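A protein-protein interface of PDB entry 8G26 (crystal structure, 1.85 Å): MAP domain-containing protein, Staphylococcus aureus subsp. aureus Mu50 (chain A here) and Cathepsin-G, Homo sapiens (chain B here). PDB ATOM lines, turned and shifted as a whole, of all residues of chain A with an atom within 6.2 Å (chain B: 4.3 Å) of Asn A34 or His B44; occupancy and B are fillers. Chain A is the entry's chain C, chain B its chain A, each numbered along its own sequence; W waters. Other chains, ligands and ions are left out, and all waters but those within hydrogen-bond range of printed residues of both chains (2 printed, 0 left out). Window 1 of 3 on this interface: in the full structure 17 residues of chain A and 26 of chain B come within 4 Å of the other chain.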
ATOM      1  N   TYR A  23      15.091  15.978  22.360  1.00  0.00           N
ATOM      2  CA  TYR A  23      14.991  14.530  22.233  1.00  0.00           C
ATOM      3  C   TYR A  23      14.025  14.185  21.111  1.00  0.00           C
ATOM      4  O   TYR A  23      13.210  15.001  20.676  1.00  0.00           O
ATOM      5  CB  TYR A  23      14.545  13.842  23.539  1.00  0.00           C
ATOM      6  CG  TYR A  23      13.137  14.139  23.905  1.00  0.00           C
ATOM      7  CD1 TYR A  23      12.090  13.407  23.351  1.00  0.00           C
ATOM      8  CD2 TYR A  23      12.827  15.186  24.765  1.00  0.00           C
ATOM      9  CE1 TYR A  23      10.766  13.705  23.646  1.00  0.00           C
ATOM     10  CE2 TYR A  23      11.506  15.479  25.078  1.00  0.00           C
ATOM     11  CZ  TYR A  23      10.476  14.730  24.505  1.00  0.00           C
ATOM     12  OH  TYR A  23       9.168  14.995  24.784  1.00  0.00           O
ATOM     13  N   ALA A  32       6.518  11.431  15.772  1.00  0.00           N
ATOM     14  CA  ALA A  32       5.728  12.654  15.701  1.00  0.00           C
ATOM     15  C   ALA A  32       6.635  13.814  15.304  1.00  0.00           C
ATOM     16  O   ALA A  32       7.809  13.848  15.654  1.00  0.00           O
ATOM     17  CB  ALA A  32       5.067  12.939  17.050  1.00  0.00           C
ATOM     18  N   PHE A  33       6.085  14.776  14.576  1.00  0.00           N
ATOM     19  CA  PHE A  33       6.880  15.890  14.074  1.00  0.00           C
ATOM     20  C   PHE A  33       6.793  17.153  14.948  1.00  0.00           C
ATOM     21  O   PHE A  33       6.889  18.266  14.432  1.00  0.00           O
ATOM     22  CB  PHE A  33       6.474  16.177  12.627  1.00  0.00           C
ATOM     23  CG  PHE A  33       7.067  15.199  11.618  1.00  0.00           C
ATOM     24  CD1 PHE A  33       8.106  14.344  11.981  1.00  0.00           C
ATOM     25  CD2 PHE A  33       6.606  15.153  10.320  1.00  0.00           C
ATOM     26  CE1 PHE A  33       8.654  13.452  11.068  1.00  0.00           C
ATOM     27  CE2 PHE A  33       7.169  14.265   9.384  1.00  0.00           C
ATOM     28  CZ  PHE A  33       8.202  13.429   9.764  1.00  0.00           C
ATOM     29  N   ASN A  34       6.639  17.010  16.260  1.00  0.00           N
ATOM     30  CA  ASN A  34       6.894  18.156  17.124  1.00  0.00           C
ATOM     31  C   ASN A  34       8.409  18.300  17.339  1.00  0.00           C
ATOM     32  O   ASN A  34       9.212  17.472  16.923  1.00  0.00           O
ATOM     33  CB  ASN A  34       6.151  18.038  18.453  1.00  0.00           C
ATOM     34  CG  ASN A  34       6.435  16.740  19.190  1.00  0.00           C
ATOM     35  OD1 ASN A  34       6.942  15.775  18.623  1.00  0.00           O
ATOM     36  ND2 ASN A  34       6.082  16.708  20.471  1.00  0.00           N
ATOM     37  N   GLN A  35       8.801  19.381  17.986  1.00  0.00           N
ATOM     38  CA  GLN A  35      10.204  19.612  18.344  1.00  0.00           C
ATOM     39  C   GLN A  35      10.210  19.715  19.859  1.00  0.00           C
ATOM     40  O   GLN A  35       9.716  20.699  20.403  1.00  0.00           O
ATOM     41  CB  GLN A  35      10.734  20.875  17.659  1.00  0.00           C
ATOM     42  CG  GLN A  35      12.167  21.203  18.028  1.00  0.00           C
ATOM     43  CD  GLN A  35      12.891  22.078  17.009  1.00  0.00           C
ATOM     44  OE1 GLN A  35      14.118  21.990  16.894  1.00  0.00           O
ATOM     45  NE2 GLN A  35      12.154  22.923  16.287  1.00  0.00           N
ATOM     46  N   SER A  36      10.709  18.685  20.548  1.00  0.00           N
ATOM     47  CA  SER A  36      10.540  18.639  21.997  1.00  0.00           C
ATOM     48  C   SER A  36      11.861  18.588  22.756  1.00  0.00           C
ATOM     49  O   SER A  36      12.895  18.141  22.246  1.00  0.00           O
ATOM     50  CB  SER A  36       9.691  17.425  22.394  1.00  0.00           C
ATOM     51  OG  SER A  36      10.270  16.265  21.818  1.00  0.00           O
ATOM     52  N   GLU A  62       4.435  10.312  26.389  1.00  0.00           N
ATOM     53  CA  GLU A  62       4.394  10.827  25.026  1.00  0.00           C
ATOM     54  C   GLU A  62       3.862   9.816  24.020  1.00  0.00           C
ATOM     55  O   GLU A  62       3.185  10.197  23.056  1.00  0.00           O
ATOM     56  CB  GLU A  62       5.794  11.254  24.566  1.00  0.00           C
ATOM     57  CG  GLU A  62       6.495  12.237  25.503  1.00  0.00           C
ATOM     58  CD  GLU A  62       6.028  13.652  25.298  1.00  0.00           C
ATOM     59  OE1 GLU A  62       6.222  14.180  24.182  1.00  0.00           O
ATOM     60  OE2 GLU A  62       5.450  14.230  26.248  1.00  0.00           O
ATOM     61  N   SER B  27       7.775  21.876  24.094  1.00  0.00           N
ATOM     62  CA  SER B  27       7.654  21.522  22.694  1.00  0.00           C
ATOM     63  C   SER B  27       7.330  22.770  21.891  1.00  0.00           C
ATOM     64  O   SER B  27       6.827  23.764  22.414  1.00  0.00           O
ATOM     65  CB  SER B  27       6.569  20.459  22.460  1.00  0.00           C
ATOM     66  OG  SER B  27       6.782  19.345  23.307  1.00  0.00           O
ATOM     67  N   ARG B  28       7.651  22.707  20.609  1.00  0.00           N
ATOM     68  CA  ARG B  28       7.299  23.733  19.638  1.00  0.00           C
ATOM     69  C   ARG B  28       6.519  23.048  18.530  1.00  0.00           C
ATOM     70  O   ARG B  28       6.901  21.960  18.072  1.00  0.00           O
ATOM     71  CB  ARG B  28       8.535  24.442  19.093  1.00  0.00           C
ATOM     72  CG  ARG B  28       9.569  24.837  20.158  1.00  0.00           C
ATOM     73  CD  ARG B  28       9.333  26.202  20.805  1.00  0.00           C
ATOM     74  NE  ARG B  28       8.587  26.132  22.058  1.00  0.00           N
ATOM     75  CZ  ARG B  28       9.123  25.935  23.258  1.00  0.00           C
ATOM     76  NH1 ARG B  28      10.433  25.776  23.419  1.00  0.00           N
ATOM     77  NH2 ARG B  28       8.324  25.883  24.321  1.00  0.00           N
ATOM     78  N   CYS B  29       5.415  23.661  18.130  1.00  0.00           N
ATOM     79  CA  CYS B  29       4.576  23.117  17.074  1.00  0.00           C
ATOM     80  C   CYS B  29       4.062  24.270  16.227  1.00  0.00           C
ATOM     81  O   CYS B  29       4.237  25.435  16.569  1.00  0.00           O
ATOM     82  CB  CYS B  29       3.369  22.329  17.623  1.00  0.00           C
ATOM     83  SG  CYS B  29       3.753  20.650  18.192  1.00  0.00           S
ATOM     84  N   ALA B  42      -2.190  19.622  16.223  1.00  0.00           N
ATOM     85  CA  ALA B  42      -2.123  18.176  16.480  1.00  0.00           C
ATOM     86  C   ALA B  42      -2.248  17.897  17.976  1.00  0.00           C
ATOM     87  O   ALA B  42      -1.766  18.676  18.796  1.00  0.00           O
ATOM     88  CB  ALA B  42      -0.804  17.600  15.967  1.00  0.00           C
ATOM     89  N   ALA B  43      -2.887  16.768  18.330  1.00  0.00           N
ATOM     90  CA  ALA B  43      -3.044  16.438  19.742  1.00  0.00           C
ATOM     91  C   ALA B  43      -1.718  16.096  20.424  1.00  0.00           C
ATOM     92  O   ALA B  43      -1.610  16.188  21.654  1.00  0.00           O
ATOM     93  CB  ALA B  43      -4.007  15.269  19.929  1.00  0.00           C
ATOM     94  N   HIS B  44      -0.730  15.612  19.676  1.00  0.00           N
ATOM     95  CA  HIS B  44       0.532  15.268  20.337  1.00  0.00           C
ATOM     96  C   HIS B  44       1.324  16.509  20.735  1.00  0.00           C
ATOM     97  O   HIS B  44       2.358  16.388  21.402  1.00  0.00           O
ATOM     98  CB  HIS B  44       1.370  14.330  19.449  1.00  0.00           C
ATOM     99  CG  HIS B  44       1.919  14.965  18.214  1.00  0.00           C
ATOM    100  ND1 HIS B  44       1.404  14.731  16.961  1.00  0.00           N
ATOM    101  CD2 HIS B  44       2.964  15.812  18.038  1.00  0.00           C
ATOM    102  CE1 HIS B  44       2.096  15.415  16.069  1.00  0.00           C
ATOM    103  NE2 HIS B  44       3.057  16.071  16.694  1.00  0.00           N
ATOM    104  N   CYS B  45       0.861  17.690  20.345  1.00  0.00           N
ATOM    105  CA  CYS B  45       1.438  18.966  20.757  1.00  0.00           C
ATOM    106  C   CYS B  45       0.886  19.461  22.099  1.00  0.00           C
ATOM    107  O   CYS B  45       1.284  20.533  22.566  1.00  0.00           O
ATOM    108  CB  CYS B  45       1.179  20.015  19.657  1.00  0.00           C
ATOM    109  SG  CYS B  45       1.965  19.645  18.053  1.00  0.00           S
ATOM    110  N   TRP B  46       0.003  18.694  22.738  1.00  0.00           N
ATOM    111  CA  TRP B  46      -0.651  19.142  23.962  1.00  0.00           C
ATOM    112  C   TRP B  46       0.365  19.291  25.090  1.00  0.00           C
ATOM    113  O   TRP B  46       1.410  18.644  25.108  1.00  0.00           O
ATOM    114  CB  TRP B  46      -1.765  18.156  24.337  1.00  0.00           C
ATOM    115  CG  TRP B  46      -2.470  18.465  25.618  1.00  0.00           C
ATOM    116  CD1 TRP B  46      -3.546  19.251  25.784  1.00  0.00           C
ATOM    117  CD2 TRP B  46      -2.120  17.972  26.929  1.00  0.00           C
ATOM    118  NE1 TRP B  46      -3.904  19.296  27.110  1.00  0.00           N
ATOM    119  CE2 TRP B  46      -3.043  18.506  27.829  1.00  0.00           C
ATOM    120  CE3 TRP B  46      -1.133  17.102  27.403  1.00  0.00           C
ATOM    121  CZ2 TRP B  46      -2.998  18.232  29.195  1.00  0.00           C
ATOM    122  CZ3 TRP B  46      -1.085  16.839  28.762  1.00  0.00           C
ATOM    123  CH2 TRP B  46      -2.008  17.402  29.635  1.00  0.00           C
ATOM    124  N   TYR B  80      -7.978  10.350  20.850  1.00  0.00           N
ATOM    125  CA  TYR B  80      -6.568  10.453  20.505  1.00  0.00           C
ATOM    126  C   TYR B  80      -5.824   9.228  21.015  1.00  0.00           C
ATOM    127  O   TYR B  80      -5.964   8.846  22.179  1.00  0.00           O
ATOM    128  CB  TYR B  80      -5.992  11.737  21.104  1.00  0.00           C
ATOM    129  CG  TYR B  80      -4.476  11.802  21.061  1.00  0.00           C
ATOM    130  CD1 TYR B  80      -3.811  11.691  19.867  1.00  0.00           C
ATOM    131  CD2 TYR B  80      -3.731  11.953  22.226  1.00  0.00           C
ATOM    132  CE1 TYR B  80      -2.417  11.728  19.812  1.00  0.00           C
ATOM    133  CE2 TYR B  80      -2.338  12.007  22.183  1.00  0.00           C
ATOM    134  CZ  TYR B  80      -1.697  11.894  20.960  1.00  0.00           C
ATOM    135  OH  TYR B  80      -0.310  11.911  20.860  1.00  0.00           O
ATOM    136  N   ILE B  85      -0.542   7.319  17.136  1.00  0.00           N
ATOM    137  CA  ILE B  85      -0.749   8.683  16.674  1.00  0.00           C
ATOM    138  C   ILE B  85      -1.959   8.715  15.732  1.00  0.00           C
ATOM    139  O   ILE B  85      -1.869   9.154  14.580  1.00  0.00           O
ATOM    140  CB  ILE B  85       0.489   9.292  16.013  1.00  0.00           C
ATOM    141  CG1 ILE B  85       1.747   8.970  16.834  1.00  0.00           C
ATOM    142  CG2 ILE B  85       0.320  10.785  15.933  1.00  0.00           C
ATOM    143  CD1 ILE B  85       2.954   9.775  16.407  1.00  0.00           C
ATOM    144  N   ASP B  88      -5.360  12.408  15.750  1.00  0.00           N
ATOM    145  CA  ASP B  88      -4.325  13.333  16.212  1.00  0.00           C
ATOM    146  C   ASP B  88      -4.753  14.760  15.879  1.00  0.00           C
ATOM    147  O   ASP B  88      -4.268  15.395  14.940  1.00  0.00           O
ATOM    148  CB  ASP B  88      -2.984  12.985  15.574  1.00  0.00           C
ATOM    149  CG  ASP B  88      -1.829  13.810  16.148  1.00  0.00           C
ATOM    150  OD1 ASP B  88      -1.987  14.402  17.237  1.00  0.00           O
ATOM    151  OD2 ASP B  88      -0.751  13.883  15.508  1.00  0.00           O
ATOM    152  N   LYS B 178      10.561  18.043  11.941  1.00  0.00           N
ATOM    153  CA  LYS B 178      10.413  18.330  13.360  1.00  0.00           C
ATOM    154  C   LYS B 178      10.132  19.803  13.622  1.00  0.00           C
ATOM    155  O   LYS B 178      10.896  20.676  13.211  1.00  0.00           O
ATOM    156  CB  LYS B 178      11.686  17.913  14.098  1.00  0.00           C
ATOM    157  CG  LYS B 178      11.895  16.417  14.114  1.00  0.00           C
ATOM    158  CD  LYS B 178      13.059  16.023  15.020  1.00  0.00           C
ATOM    159  CE  LYS B 178      14.395  16.422  14.431  1.00  0.00           C
ATOM    160  NZ  LYS B 178      15.451  15.422  14.768  1.00  0.00           N
ATOM    161  N   GLY B 179       9.068  20.069  14.370  1.00  0.00           N
ATOM    162  CA  GLY B 179       8.596  21.422  14.606  1.00  0.00           C
ATOM    163  C   GLY B 179       7.448  21.845  13.708  1.00  0.00           C
ATOM    164  O   GLY B 179       6.796  22.861  13.998  1.00  0.00           O
ATOM    165  N   SER B 181       4.703  19.856  13.069  1.00  0.00           N
ATOM    166  CA  SER B 181       3.447  19.254  13.501  1.00  0.00           C
ATOM    167  C   SER B 181       2.425  20.328  13.800  1.00  0.00           C
ATOM    168  O   SER B 181       2.754  21.369  14.368  1.00  0.00           O
ATOM    169  CB  SER B 181       3.656  18.425  14.780  1.00  0.00           C
ATOM    170  OG  SER B 181       4.057  17.095  14.494  1.00  0.00           O
ATOM    171  N   SER B 196       1.266  15.525  11.023  1.00  0.00           N
ATOM    172  CA  SER B 196       1.243  14.625  12.177  1.00  0.00           C
ATOM    173  C   SER B 196       2.535  13.847  12.398  1.00  0.00           C
ATOM    174  O   SER B 196       3.222  14.095  13.401  1.00  0.00           O
ATOM    175  CB  SER B 196       0.044  13.664  12.006  1.00  0.00           C
ATOM    176  OG  SER B 196      -0.091  12.770  13.107  1.00  0.00           O
HETATM  177  O   HOH W   1       1.220  12.189  23.104  1.00  0.00           O
HETATM  178  O   HOH W   2       3.321  14.216  22.665  1.00  0.00           O
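Of chain B, only Ser B27 (3.9 Å), Arg B28 (3.9 Å), Cys B29 (3.6 Å), His B44 (3.7 Å), Lys B178 (3.8 Å), Gly B179 (3.5 Å) and Ser B181 (3.1 Å) come within 4 Å of Asn A34. Of the printed residues of chain B, Ser A36 touches Ser B27. Glu A62 touches none of the printed residues of chain B. Of the printed residues of chain A, Cys B29 touches Asn A34. Ala B43 touches none of the printed residues of chain A. His B44 touches three residues of chain A. Printed residues of chain A within 4 Å of Ile B85: Ala A32. Of the printed residues of chain A, Lys B178 touches Phe A33 and Asn A34. Of the printed residues of chain A, Ser B196 touches Ala A32 (3.7 Å) and Phe A33 (3.2 Å).
The backbone carbonyl oxygen (O) of Gln A35 lies within hydrogen-bond range of the backbone NH (N) of Arg B28 (2.9 Å). O of Phe A33 sits at hydrogen-bond distance from N of Gly B179, at 2.8 Å. The backbone carbonyl oxygen (O) of Phe A33 lies within hydrogen-bond range of the backbone NH (N) of Ser B181 (3.0 Å). The backbone NH (N) of Asn A34 lies within hydrogen-bond range of the side-chain hydroxyl (OG) of Ser B181. The backbone carbonyl oxygen (O) of Ser B196 sits at hydrogen-bond distance from the backbone NH (N) of Phe A33 (3.2 Å).
Among the printed residues, merely in contact across the chains: Gln A35 with Ser B27, Asn A34 with Gly B179, Asn A34 with Cys B29, Ser A36 with Ser B27, Phe A33 with Lys B178, Gln A35 with Gly B179, Ala A32 with Ser B196, Ala A32 with His B44, Asn A34 with His B44, Asn A34 with Lys B178, Ala A32 with Ile B85, Phe A33 with His B44, Asn A34 with Arg B28 and Asn A34 with Ser B27.
The side-chain sulfur (SG) of Cys B45 is disulfide-bonded to the side-chain sulfur (SG) of Cys B29, at 2.1 Å. A ring nitrogen (ND1) of His B44 lies within hydrogen-bond range of the side-chain carboxylate of Asp B88 (2.7 Å). OG of Ser B181 is in hydrogen-bond range of NE2 of His B44, at 2.6 Å. OG of Ser B196 sits at hydrogen-bond distance from OD2 of Asp B88. OG of Ser B181 sits at hydrogen-bond distance from O of Ser B196, 3.3 Å away. N of Tyr A23 lies within hydrogen-bond range of O of Ser A36 (3.1 Å).
Of the 15 printed residues of chain B, 9 touch a printed residue of chain A. Hydrophobic or aromatic side chains of chain B that line the printed part of chain A: His B44 and Ile B85. Of the 7 printed residues of chain A, 5 touch a printed residue of chain B. Among the printed residues, no Asp or Glu carboxylate lies within 4 Å of a Lys or Arg side-chain nitrogen of the other chain.
Water W2 lies within hydrogen-bond range of the backbone carbonyl oxygen (O) of His B44 and the side-chain carboxylate (OE1) of Glu A62. Water W1 lies within hydrogen-bond range of OH of Tyr B80 (2.7 Å) and O of Glu A62 (2.8 Å).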
